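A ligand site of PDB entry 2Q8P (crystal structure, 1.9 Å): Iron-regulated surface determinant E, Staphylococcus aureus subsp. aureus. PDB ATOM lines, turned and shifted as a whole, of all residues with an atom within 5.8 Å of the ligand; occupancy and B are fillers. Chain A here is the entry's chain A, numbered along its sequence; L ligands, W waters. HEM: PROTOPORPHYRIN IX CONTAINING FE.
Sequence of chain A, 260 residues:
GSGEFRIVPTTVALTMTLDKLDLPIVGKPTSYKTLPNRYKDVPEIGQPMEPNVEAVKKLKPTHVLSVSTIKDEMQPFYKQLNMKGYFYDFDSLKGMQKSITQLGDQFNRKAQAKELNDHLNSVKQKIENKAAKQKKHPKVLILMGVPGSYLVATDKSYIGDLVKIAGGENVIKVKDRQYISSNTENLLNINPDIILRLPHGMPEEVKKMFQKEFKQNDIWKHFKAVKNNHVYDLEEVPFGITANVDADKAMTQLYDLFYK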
ATOM      1  N   THR A  10      34.312  -8.602 -14.986  1.00  0.00           N
ATOM      2  CA  THR A  10      33.286  -9.633 -14.931  1.00  0.00           C
ATOM      3  C   THR A  10      31.999  -9.125 -14.270  1.00  0.00           C
ATOM      4  O   THR A  10      31.019  -9.867 -14.193  1.00  0.00           O
ATOM      5  CB  THR A  10      33.790 -10.953 -14.260  1.00  0.00           C
ATOM      6  OG1 THR A  10      34.206 -10.704 -12.902  1.00  0.00           O
ATOM      7  CG2 THR A  10      34.987 -11.503 -15.040  1.00  0.00           C
ATOM      8  N   THR A  11      32.007  -7.887 -13.773  1.00  0.00           N
ATOM      9  CA  THR A  11      30.796  -7.367 -13.158  1.00  0.00           C
ATOM     10  C   THR A  11      30.353  -6.076 -13.831  1.00  0.00           C
ATOM     11  O   THR A  11      31.158  -5.390 -14.468  1.00  0.00           O
ATOM     12  CB  THR A  11      30.942  -7.162 -11.621  1.00  0.00           C
ATOM     13  OG1 THR A  11      31.725  -5.994 -11.354  1.00  0.00           O
ATOM     14  CG2 THR A  11      31.615  -8.378 -10.928  1.00  0.00           C
ATOM     15  N   VAL A  12      29.077  -5.743 -13.689  1.00  0.00           N
ATOM     16  CA  VAL A  12      28.540  -4.515 -14.290  1.00  0.00           C
ATOM     17  C   VAL A  12      29.166  -3.297 -13.598  1.00  0.00           C
ATOM     18  O   VAL A  12      29.495  -2.320 -14.255  1.00  0.00           O
ATOM     19  CB  VAL A  12      27.011  -4.484 -14.216  1.00  0.00           C
ATOM     20  CG1 VAL A  12      26.438  -3.109 -14.670  1.00  0.00           C
ATOM     21  CG2 VAL A  12      26.414  -5.630 -15.033  1.00  0.00           C
ATOM     22  N   ALA A  13      29.347  -3.358 -12.273  1.00  0.00           N
ATOM     23  CA  ALA A  13      30.003  -2.241 -11.562  1.00  0.00           C
ATOM     24  C   ALA A  13      31.415  -2.002 -12.077  1.00  0.00           C
ATOM     25  O   ALA A  13      31.787  -0.852 -12.414  1.00  0.00           O
ATOM     26  CB  ALA A  13      29.952  -2.447 -10.030  1.00  0.00           C
ATOM     27  N   LEU A  14      32.209  -3.074 -12.204  1.00  0.00           N
ATOM     28  CA  LEU A  14      33.552  -2.938 -12.803  1.00  0.00           C
ATOM     29  C   LEU A  14      33.544  -2.361 -14.216  1.00  0.00           C
ATOM     30  O   LEU A  14      34.377  -1.526 -14.557  1.00  0.00           O
ATOM     31  CB  LEU A  14      34.311  -4.264 -12.771  1.00  0.00           C
ATOM     32  CG  LEU A  14      34.868  -4.638 -11.410  1.00  0.00           C
ATOM     33  CD1 LEU A  14      35.073  -6.149 -11.348  1.00  0.00           C
ATOM     34  CD2 LEU A  14      36.176  -3.903 -11.124  1.00  0.00           C
ATOM     35  N   PRO A  29      30.380  -8.481 -18.946  1.00  0.00           N
ATOM     36  CA  PRO A  29      29.395  -9.411 -18.401  1.00  0.00           C
ATOM     37  C   PRO A  29      28.102  -9.495 -19.211  1.00  0.00           C
ATOM     38  O   PRO A  29      27.723  -8.546 -19.913  1.00  0.00           O
ATOM     39  CB  PRO A  29      29.097  -8.833 -17.013  1.00  0.00           C
ATOM     40  CG  PRO A  29      29.562  -7.483 -17.026  1.00  0.00           C
ATOM     41  CD  PRO A  29      30.640  -7.357 -18.036  1.00  0.00           C
ATOM     42  N   THR A  30      27.446 -10.642 -19.099  1.00  0.00           N
ATOM     43  CA  THR A  30      26.110 -10.828 -19.643  1.00  0.00           C
ATOM     44  C   THR A  30      25.122 -10.286 -18.615  1.00  0.00           C
ATOM     45  O   THR A  30      25.048 -10.765 -17.507  1.00  0.00           O
ATOM     46  CB  THR A  30      25.809 -12.313 -19.904  1.00  0.00           C
ATOM     47  OG1 THR A  30      26.822 -12.869 -20.759  1.00  0.00           O
ATOM     48  CG2 THR A  30      24.444 -12.462 -20.561  1.00  0.00           C
ATOM     49  N   SER A  31      24.374  -9.246 -18.985  1.00  0.00           N
ATOM     50  CA  SER A  31      23.536  -8.567 -18.007  1.00  0.00           C
ATOM     51  C   SER A  31      22.277  -8.049 -18.680  1.00  0.00           C
ATOM     52  O   SER A  31      22.293  -7.699 -19.877  1.00  0.00           O
ATOM     53  CB  SER A  31      24.319  -7.410 -17.340  1.00  0.00           C
ATOM     54  OG  SER A  31      23.535  -6.701 -16.395  1.00  0.00           O
ATOM     55  N   TYR A  32      21.192  -7.980 -17.917  1.00  0.00           N
ATOM     56  CA  TYR A  32      20.013  -7.229 -18.330  1.00  0.00           C
ATOM     57  C   TYR A  32      20.163  -5.723 -18.130  1.00  0.00           C
ATOM     58  O   TYR A  32      19.304  -4.958 -18.599  1.00  0.00           O
ATOM     59  CB  TYR A  32      18.717  -7.755 -17.654  1.00  0.00           C
ATOM     60  CG  TYR A  32      18.762  -7.772 -16.152  1.00  0.00           C
ATOM     61  CD1 TYR A  32      18.796  -8.977 -15.476  1.00  0.00           C
ATOM     62  CD2 TYR A  32      18.772  -6.589 -15.408  1.00  0.00           C
ATOM     63  CE1 TYR A  32      18.848  -9.011 -14.096  1.00  0.00           C
ATOM     64  CE2 TYR A  32      18.824  -6.610 -14.017  1.00  0.00           C
ATOM     65  CZ  TYR A  32      18.869  -7.835 -13.370  1.00  0.00           C
ATOM     66  OH  TYR A  32      18.904  -7.920 -12.002  1.00  0.00           O
ATOM     67  N   LYS A  33      21.242  -5.279 -17.470  1.00  0.00           N
ATOM     68  CA  LYS A  33      21.431  -3.849 -17.173  1.00  0.00           C
ATOM     69  C   LYS A  33      22.065  -3.130 -18.340  1.00  0.00           C
ATOM     70  O   LYS A  33      22.709  -3.747 -19.189  1.00  0.00           O
ATOM     71  CB  LYS A  33      22.281  -3.629 -15.918  1.00  0.00           C
ATOM     72  CG  LYS A  33      21.698  -4.287 -14.690  1.00  0.00           C
ATOM     73  CD  LYS A  33      22.628  -4.176 -13.493  1.00  0.00           C
ATOM     74  CE  LYS A  33      21.975  -4.783 -12.271  1.00  0.00           C
ATOM     75  NZ  LYS A  33      22.995  -5.022 -11.200  1.00  0.00           N
ATOM     76  N   GLN A  47      27.347 -14.563 -16.926  1.00  0.00           N
ATOM     77  CA  GLN A  47      26.821 -13.775 -15.814  1.00  0.00           C
ATOM     78  C   GLN A  47      27.906 -13.546 -14.751  1.00  0.00           C
ATOM     79  O   GLN A  47      28.757 -14.395 -14.545  1.00  0.00           O
ATOM     80  CB  GLN A  47      25.544 -14.389 -15.229  1.00  0.00           C
ATOM     81  CG  GLN A  47      25.756 -15.528 -14.242  1.00  0.00           C
ATOM     82  CD  GLN A  47      25.289 -15.179 -12.812  1.00  0.00           C
ATOM     83  OE1 GLN A  47      25.617 -14.118 -12.260  1.00  0.00           O
ATOM     84  NE2 GLN A  47      24.499 -16.073 -12.237  1.00  0.00           N
ATOM     85  N   PRO A  48      27.917 -12.349 -14.138  1.00  0.00           N
ATOM     86  CA  PRO A  48      28.952 -11.968 -13.179  1.00  0.00           C
ATOM     87  C   PRO A  48      29.402 -13.060 -12.199  1.00  0.00           C
ATOM     88  O   PRO A  48      30.608 -13.232 -11.974  1.00  0.00           O
ATOM     89  CB  PRO A  48      28.329 -10.788 -12.455  1.00  0.00           C
ATOM     90  CG  PRO A  48      27.567 -10.089 -13.558  1.00  0.00           C
ATOM     91  CD  PRO A  48      26.970 -11.235 -14.376  1.00  0.00           C
ATOM     92  N   MET A  49      28.457 -13.796 -11.639  1.00  0.00           N
ATOM     93  CA  MET A  49      28.784 -14.791 -10.621  1.00  0.00           C
ATOM     94  C   MET A  49      29.301 -16.108 -11.181  1.00  0.00           C
ATOM     95  O   MET A  49      29.839 -16.923 -10.430  1.00  0.00           O
ATOM     96  CB  MET A  49      27.553 -15.068  -9.781  1.00  0.00           C
ATOM     97  CG  MET A  49      27.079 -13.868  -9.009  1.00  0.00           C
ATOM     98  SD  MET A  49      25.541 -14.455  -7.993  1.00  0.00           S
ATOM     99  CE  MET A  49      26.462 -15.322  -6.512  1.00  0.00           C
ATOM    100  N   VAL A  67      35.170  -8.881  -7.840  1.00  0.00           N
ATOM    101  CA  VAL A  67      34.947  -8.047  -6.647  1.00  0.00           C
ATOM    102  C   VAL A  67      35.020  -8.823  -5.339  1.00  0.00           C
ATOM    103  O   VAL A  67      34.694 -10.014  -5.288  1.00  0.00           O
ATOM    104  CB  VAL A  67      33.594  -7.246  -6.707  1.00  0.00           C
ATOM    105  CG1 VAL A  67      33.622  -6.198  -7.851  1.00  0.00           C
ATOM    106  CG2 VAL A  67      32.369  -8.195  -6.790  1.00  0.00           C
ATOM    107  N   THR A  69      33.037  -8.947  -2.875  1.00  0.00           N
ATOM    108  CA  THR A  69      31.738  -9.460  -2.397  1.00  0.00           C
ATOM    109  C   THR A  69      31.519 -10.957  -2.696  1.00  0.00           C
ATOM    110  O   THR A  69      30.813 -11.662  -1.967  1.00  0.00           O
ATOM    111  CB  THR A  69      30.604  -8.654  -3.039  1.00  0.00           C
ATOM    112  OG1 THR A  69      30.960  -7.257  -3.080  1.00  0.00           O
ATOM    113  CG2 THR A  69      29.268  -8.831  -2.278  1.00  0.00           C
ATOM    114  N   ILE A  70      32.126 -11.421  -3.774  1.00  0.00           N
ATOM    115  CA  ILE A  70      32.002 -12.835  -4.158  1.00  0.00           C
ATOM    116  C   ILE A  70      33.380 -13.511  -4.329  1.00  0.00           C
ATOM    117  O   ILE A  70      33.517 -14.445  -5.102  1.00  0.00           O
ATOM    118  CB  ILE A  70      31.142 -12.992  -5.433  1.00  0.00           C
ATOM    119  CG1 ILE A  70      31.567 -11.972  -6.515  1.00  0.00           C
ATOM    120  CG2 ILE A  70      29.676 -12.803  -5.074  1.00  0.00           C
ATOM    121  CD1 ILE A  70      30.996 -12.279  -7.905  1.00  0.00           C
ATOM    122  N   VAL A 146      16.997 -12.020  -2.979  1.00  0.00           N
ATOM    123  CA  VAL A 146      17.640 -12.768  -4.047  1.00  0.00           C
ATOM    124  C   VAL A 146      16.631 -13.829  -4.518  1.00  0.00           C
ATOM    125  O   VAL A 146      15.605 -14.061  -3.842  1.00  0.00           O
ATOM    126  CB  VAL A 146      18.954 -13.431  -3.532  1.00  0.00           C
ATOM    127  CG1 VAL A 146      19.964 -12.378  -3.096  1.00  0.00           C
ATOM    128  CG2 VAL A 146      18.684 -14.386  -2.383  1.00  0.00           C
ATOM    129  N   PRO A 147      16.883 -14.463  -5.677  1.00  0.00           N
ATOM    130  CA  PRO A 147      15.974 -15.559  -6.080  1.00  0.00           C
ATOM    131  C   PRO A 147      15.846 -16.621  -4.991  1.00  0.00           C
ATOM    132  O   PRO A 147      16.853 -17.195  -4.572  1.00  0.00           O
ATOM    133  CB  PRO A 147      16.657 -16.124  -7.331  1.00  0.00           C
ATOM    134  CG  PRO A 147      17.382 -14.923  -7.899  1.00  0.00           C
ATOM    135  CD  PRO A 147      17.942 -14.226  -6.692  1.00  0.00           C
ATOM    136  N   SER A 149      14.880 -16.352  -1.687  1.00  0.00           N
ATOM    137  CA  SER A 149      14.949 -15.929  -0.285  1.00  0.00           C
ATOM    138  C   SER A 149      15.380 -14.479  -0.115  1.00  0.00           C
ATOM    139  O   SER A 149      15.813 -13.846  -1.061  1.00  0.00           O
ATOM    140  CB  SER A 149      15.925 -16.846   0.482  1.00  0.00           C
ATOM    141  OG  SER A 149      17.225 -16.734  -0.090  1.00  0.00           O
ATOM    142  N   LEU A 151      17.874 -11.892   2.484  1.00  0.00           N
ATOM    143  CA  LEU A 151      18.892 -11.718   3.495  1.00  0.00           C
ATOM    144  C   LEU A 151      18.732 -10.343   4.115  1.00  0.00           C
ATOM    145  O   LEU A 151      17.942  -9.516   3.636  1.00  0.00           O
ATOM    146  CB  LEU A 151      20.260 -11.829   2.818  1.00  0.00           C
ATOM    147  CG  LEU A 151      20.438 -13.092   1.949  1.00  0.00           C
ATOM    148  CD1 LEU A 151      21.492 -12.902   0.856  1.00  0.00           C
ATOM    149  CD2 LEU A 151      20.727 -14.300   2.761  1.00  0.00           C
ATOM    150  N   GLN A 178      28.632  -9.043   4.812  1.00  0.00           N
ATOM    151  CA  GLN A 178      27.829  -8.053   4.077  1.00  0.00           C
ATOM    152  C   GLN A 178      26.323  -8.320   4.229  1.00  0.00           C
ATOM    153  O   GLN A 178      25.546  -7.411   4.515  1.00  0.00           O
ATOM    154  CB  GLN A 178      28.220  -8.052   2.590  1.00  0.00           C
ATOM    155  CG  GLN A 178      29.653  -7.649   2.326  1.00  0.00           C
ATOM    156  CD  GLN A 178      30.622  -8.828   2.235  1.00  0.00           C
ATOM    157  OE1 GLN A 178      30.414  -9.906   2.833  1.00  0.00           O
ATOM    158  NE2 GLN A 178      31.679  -8.634   1.470  1.00  0.00           N
ATOM    159  N   TYR A 179      25.950  -9.586   4.111  1.00  0.00           N
ATOM    160  CA  TYR A 179      24.543 -10.012   4.147  1.00  0.00           C
ATOM    161  C   TYR A 179      24.419 -11.210   5.050  1.00  0.00           C
ATOM    162  O   TYR A 179      25.231 -12.151   4.966  1.00  0.00           O
ATOM    163  CB  TYR A 179      24.047 -10.377   2.737  1.00  0.00           C
ATOM    164  CG  TYR A 179      24.228  -9.229   1.777  1.00  0.00           C
ATOM    165  CD1 TYR A 179      23.403  -8.095   1.851  1.00  0.00           C
ATOM    166  CD2 TYR A 179      25.270  -9.224   0.851  1.00  0.00           C
ATOM    167  CE1 TYR A 179      23.593  -7.008   0.970  1.00  0.00           C
ATOM    168  CE2 TYR A 179      25.468  -8.145  -0.011  1.00  0.00           C
ATOM    169  CZ  TYR A 179      24.632  -7.049   0.071  1.00  0.00           C
ATOM    170  OH  TYR A 179      24.854  -6.005  -0.770  1.00  0.00           O
ATOM    171  N   HIS A 200      17.588  -8.440  -6.257  1.00  0.00           N
ATOM    172  CA  HIS A 200      18.850  -8.873  -6.847  1.00  0.00           C
ATOM    173  C   HIS A 200      18.591 -10.060  -7.754  1.00  0.00           C
ATOM    174  O   HIS A 200      17.797 -10.912  -7.437  1.00  0.00           O
ATOM    175  CB  HIS A 200      19.867  -9.298  -5.756  1.00  0.00           C
ATOM    176  CG  HIS A 200      21.152  -9.828  -6.322  1.00  0.00           C
ATOM    177  ND1 HIS A 200      22.064  -9.037  -7.017  1.00  0.00           N
ATOM    178  CD2 HIS A 200      21.655 -11.080  -6.335  1.00  0.00           C
ATOM    179  CE1 HIS A 200      23.072  -9.792  -7.416  1.00  0.00           C
ATOM    180  NE2 HIS A 200      22.857 -11.044  -6.996  1.00  0.00           N
ATOM    181  N   GLY A 201      19.322 -10.121  -8.862  1.00  0.00           N
ATOM    182  CA  GLY A 201      19.438 -11.321  -9.672  1.00  0.00           C
ATOM    183  C   GLY A 201      18.234 -11.526 -10.580  1.00  0.00           C
ATOM    184  O   GLY A 201      18.375 -11.630 -11.793  1.00  0.00           O
ATOM    185  N   MET A 202      17.051 -11.535  -9.966  1.00  0.00           N
ATOM    186  CA  MET A 202      15.778 -11.717 -10.656  1.00  0.00           C
ATOM    187  C   MET A 202      14.731 -10.766 -10.086  1.00  0.00           C
ATOM    188  O   MET A 202      13.886 -11.178  -9.315  1.00  0.00           O
ATOM    189  CB  MET A 202      15.328 -13.157 -10.496  1.00  0.00           C
ATOM    190  CG  MET A 202      16.237 -14.155 -11.179  1.00  0.00           C
ATOM    191  SD  MET A 202      15.749 -14.235 -13.039  1.00  0.00           S
ATOM    192  CE  MET A 202      17.351 -15.094 -13.778  1.00  0.00           C
ATOM    193  N   GLU A 236      17.104  -1.507  -8.177  1.00  0.00           N
ATOM    194  CA  GLU A 236      18.407  -2.186  -8.161  1.00  0.00           C
ATOM    195  C   GLU A 236      19.511  -1.323  -8.812  1.00  0.00           C
ATOM    196  O   GLU A 236      20.700  -1.422  -8.461  1.00  0.00           O
ATOM    197  CB  GLU A 236      18.282  -3.522  -8.888  1.00  0.00           C
ATOM    198  CG  GLU A 236      19.522  -4.372  -8.757  1.00  0.00           C
ATOM    199  CD  GLU A 236      19.541  -5.548  -9.684  1.00  0.00           C
ATOM    200  OE1 GLU A 236      18.731  -5.613 -10.651  1.00  0.00           O
ATOM    201  OE2 GLU A 236      20.365  -6.439  -9.412  1.00  0.00           O
ATOM    202  N   ILE A 241      23.883  -4.625  -5.247  1.00  0.00           N
ATOM    203  CA  ILE A 241      24.467  -5.545  -4.226  1.00  0.00           C
ATOM    204  C   ILE A 241      25.950  -5.215  -3.906  1.00  0.00           C
ATOM    205  O   ILE A 241      26.505  -5.669  -2.882  1.00  0.00           O
ATOM    206  CB  ILE A 241      24.263  -7.030  -4.653  1.00  0.00           C
ATOM    207  CG1 ILE A 241      24.299  -7.974  -3.434  1.00  0.00           C
ATOM    208  CG2 ILE A 241      25.292  -7.444  -5.722  1.00  0.00           C
ATOM    209  CD1 ILE A 241      23.612  -9.381  -3.647  1.00  0.00           C
ATOM    210  N   THR A 242      26.583  -4.444  -4.781  1.00  0.00           N
ATOM    211  CA  THR A 242      27.902  -3.856  -4.520  1.00  0.00           C
ATOM    212  C   THR A 242      27.830  -2.364  -4.841  1.00  0.00           C
ATOM    213  O   THR A 242      26.887  -1.916  -5.519  1.00  0.00           O
ATOM    214  CB  THR A 242      29.054  -4.462  -5.378  1.00  0.00           C
ATOM    215  OG1 THR A 242      29.090  -3.809  -6.667  1.00  0.00           O
ATOM    216  CG2 THR A 242      28.925  -6.018  -5.531  1.00  0.00           C
ATOM    217  N   ALA A 243      28.845  -1.621  -4.410  1.00  0.00           N
ATOM    218  CA  ALA A 243      29.036  -0.240  -4.854  1.00  0.00           C
ATOM    219  C   ALA A 243      29.146  -0.154  -6.371  1.00  0.00           C
ATOM    220  O   ALA A 243      29.481  -1.142  -7.028  1.00  0.00           O
ATOM    221  CB  ALA A 243      30.263   0.383  -4.197  1.00  0.00           C
ATOM    222  N   ASN A 244      28.860   1.037  -6.902  1.00  0.00           N
ATOM    223  CA  ASN A 244      28.983   1.301  -8.315  1.00  0.00           C
ATOM    224  C   ASN A 244      29.243   2.807  -8.465  1.00  0.00           C
ATOM    225  O   ASN A 244      29.031   3.567  -7.512  1.00  0.00           O
ATOM    226  CB  ASN A 244      27.720   0.870  -9.062  1.00  0.00           C
ATOM    227  CG  ASN A 244      27.942   0.653 -10.556  1.00  0.00           C
ATOM    228  OD1 ASN A 244      27.087   0.038 -11.220  1.00  0.00           O
ATOM    229  ND2 ASN A 244      29.047   1.136 -11.090  1.00  0.00           N
HETATM  230  CHA HEM L   1      25.087 -10.631 -10.174  1.00  0.00           C
HETATM  231  CHB HEM L   1      21.957 -14.312  -9.547  1.00  0.00           C
HETATM  232  CHC HEM L   1      22.729 -14.124  -4.750  1.00  0.00           C
HETATM  233  CHD HEM L   1      26.610 -11.314  -5.567  1.00  0.00           C
HETATM  234  C1A HEM L   1      24.077 -11.548 -10.415  1.00  0.00           C
HETATM  235  C2A HEM L   1      23.286 -11.691 -11.626  1.00  0.00           C
HETATM  236  C3A HEM L   1      22.422 -12.721 -11.448  1.00  0.00           C
HETATM  237  C4A HEM L   1      22.652 -13.254 -10.127  1.00  0.00           C
HETATM  238  CMA HEM L   1      21.357 -13.271 -12.442  1.00  0.00           C
HETATM  239  CAA HEM L   1      23.405 -10.825 -12.904  1.00  0.00           C
HETATM  240  CBA HEM L   1      22.364  -9.728 -12.895  1.00  0.00           C
HETATM  241  CGA HEM L   1      22.556  -8.922 -14.156  1.00  0.00           C
HETATM  242  O1A HEM L   1      23.300  -7.878 -14.132  1.00  0.00           O
HETATM  243  O2A HEM L   1      21.957  -9.347 -15.183  1.00  0.00           O
HETATM  244  C1B HEM L   1      21.911 -14.635  -8.214  1.00  0.00           C
HETATM  245  C2B HEM L   1      21.157 -15.756  -7.606  1.00  0.00           C
HETATM  246  C3B HEM L   1      21.372 -15.732  -6.282  1.00  0.00           C
HETATM  247  C4B HEM L   1      22.250 -14.581  -5.968  1.00  0.00           C
HETATM  248  CMB HEM L   1      20.319 -16.768  -8.421  1.00  0.00           C
HETATM  249  CAB HEM L   1      20.745 -16.754  -5.286  1.00  0.00           C
HETATM  250  CBB HEM L   1      20.435 -16.443  -4.023  1.00  0.00           C
HETATM  251  C1C HEM L   1      23.878 -13.379  -4.530  1.00  0.00           C
HETATM  252  C2C HEM L   1      24.572 -13.164  -3.261  1.00  0.00           C
HETATM  253  C3C HEM L   1      25.659 -12.393  -3.510  1.00  0.00           C
HETATM  254  C4C HEM L   1      25.667 -12.076  -4.924  1.00  0.00           C
HETATM  255  CMC HEM L   1      24.140 -13.764  -1.905  1.00  0.00           C
HETATM  256  CAC HEM L   1      26.745 -11.907  -2.539  1.00  0.00           C
HETATM  257  CBC HEM L   1      26.471 -11.123  -1.500  1.00  0.00           C
HETATM  258  C1D HEM L   1      26.582 -10.857  -6.869  1.00  0.00           C
HETATM  259  C2D HEM L   1      27.557  -9.954  -7.454  1.00  0.00           C
HETATM  260  C3D HEM L   1      27.100  -9.732  -8.895  1.00  0.00           C
HETATM  261  C4D HEM L   1      25.884 -10.529  -9.047  1.00  0.00           C
HETATM  262  CMD HEM L   1      28.780  -9.357  -6.723  1.00  0.00           C
HETATM  263  CAD HEM L   1      27.784  -8.822  -9.946  1.00  0.00           C
HETATM  264  CBD HEM L   1      27.193  -7.437  -9.719  1.00  0.00           C
HETATM  265  CGD HEM L   1      27.605  -6.555 -10.872  1.00  0.00           C
HETATM  266  O1D HEM L   1      28.125  -5.429 -10.558  1.00  0.00           O
HETATM  267  O2D HEM L   1      27.425  -7.005 -12.051  1.00  0.00           O
HETATM  268  NA  HEM L   1      23.655 -12.524  -9.523  1.00  0.00           N
HETATM  269  NB  HEM L   1      22.545 -13.985  -7.180  1.00  0.00           N
HETATM  270  NC  HEM L   1      24.581 -12.694  -5.516  1.00  0.00           N
HETATM  271  ND  HEM L   1      25.638 -11.155  -7.817  1.00  0.00           N
HETATM  272 FE   HEM L   1      24.050 -12.521  -7.498  1.00  0.00          FE
HETATM  273  O   HOH W   1      21.013 -11.624 -15.798  1.00  0.00           O
HETATM  274  O   HOH W   2      26.691  -4.001  -8.495  1.00  0.00           O
HETATM  275  O   HOH W   3      18.758 -12.730 -14.546  1.00  0.00           O
HETATM  276  O   HOH W   4      17.922 -18.018  -2.220  1.00  0.00           O
HETATM  277  O   HOH W   5      24.606  -7.202 -12.149  1.00  0.00           O
HETATM  278  O   HOH W   6      30.185  -5.553  -8.829  1.00  0.00           O
HETATM  279  O   HOH W   7      19.449 -16.359 -11.718  1.00  0.00           O
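The side-chain sulfur (SD) of Met 49 binds an iron atom (FE) of the ligand, at 2.5 Å.
The backbone NH (N) of Tyr 32 lies within hydrogen-bond range of an oxygen (O2A) of the ligand.
The backbone NH of Ala 13 lies within hydrogen-bond range of an oxygen (O1D) of the ligand, at 3.0 Å.
The backbone NH (N) of Val 12 sits at hydrogen-bond distance from an oxygen (O2D) of the ligand (2.6 Å).
The side-chain hydroxyl (OG) of Ser 31 lies within hydrogen-bond range of an oxygen (O1A) of the ligand (2.6 Å).
An iron atom (FE) of the ligand is bound by a ring nitrogen (NE2) of His 200, at 2.0 Å.
The side-chain carboxylate of Glu 236 lies within hydrogen-bond range of the side-chain hydroxyl of Tyr 32 (2.7 Å).
The side-chain hydroxyl of Tyr 179 lies within hydrogen-bond range of the backbone carbonyl oxygen of Ile 241.
N of Met 49 lies within hydrogen-bond range of OE1 of Gln 47, 2.9 Å away.
The side-chain amino group (NZ) of Lys 33 is in salt-bridge range of the side-chain carboxylate (OE2) of Glu 236, at 3.5 Å.
The side-chain hydroxyl (OG) of Ser 31 lies within hydrogen-bond range of the backbone NH (N) of Lys 33, at 2.9 Å.
The side-chain hydroxyl (OG1) of Thr 11 is in hydrogen-bond range of the backbone NH (N) of Leu 14 (3.1 Å).
Thr 11 touches the ligand (CB to CGD, 3.5 Å).
Lys 33 touches the ligand (CD to O1A, 3.8 Å).
Gln 47 touches the ligand (OE1 to C2A, 3.4 Å).
Pro 48 touches the ligand.
Val 67 touches the ligand (CG2 to CMD, 3.8 Å).
Thr 69 touches the ligand.
Ile 70 touches the ligand (CG2 to CHD, 3.4 Å).
Val 146 touches the ligand (CG2 to CBB, 3.2 Å).
Pro 147 touches the ligand (CG to CMB, 3.5 Å).
Leu 151 touches the ligand.
Tyr 179 touches the ligand.
Gly 201 touches the ligand (O to CMA, 3.5 Å).
Ile 241 touches the ligand (CD1 to C4C, 3.6 Å).
Thr 242 touches the ligand.
Hydrophobic or aromatic side chains within 4 Å of the ligand: Val 12, Ala 13, Tyr 32, Pro 48, Met 49, Val 67, Ile 70, Val 146, Pro 147, Leu 151, Tyr 179, His 200 and Ile 241.
20 residues have an atom within 4 Å of the ligand: Thr 11, Val 12, Ala 13, Ser 31, Tyr 32, Lys 33, Gln 47, Pro 48, Met 49, Val 67, Thr 69, Ile 70, Val 146, Pro 147, Leu 151, Tyr 179, His 200, Gly 201, Ile 241 and Thr 242.
Water W5 bridges O1A of the ligand (2.5 Å) and NZ of Lys 33 (2.9 Å).
Water W6 lies within hydrogen-bond range of O1D of the ligand, OG1 of Thr 242 and OG1 of Thr 11.
Water W2 lies within hydrogen-bond range of O1D of the ligand (2.9 Å) and OG1 of Thr 242 (3.0 Å).
Water W3 lies within hydrogen-bond range of O of Gly 201 (3.0 Å) and SD of Met 202 (3.7 Å).
Water W4 lies within hydrogen-bond range of OG of Ser 149 and O of Pro 147.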
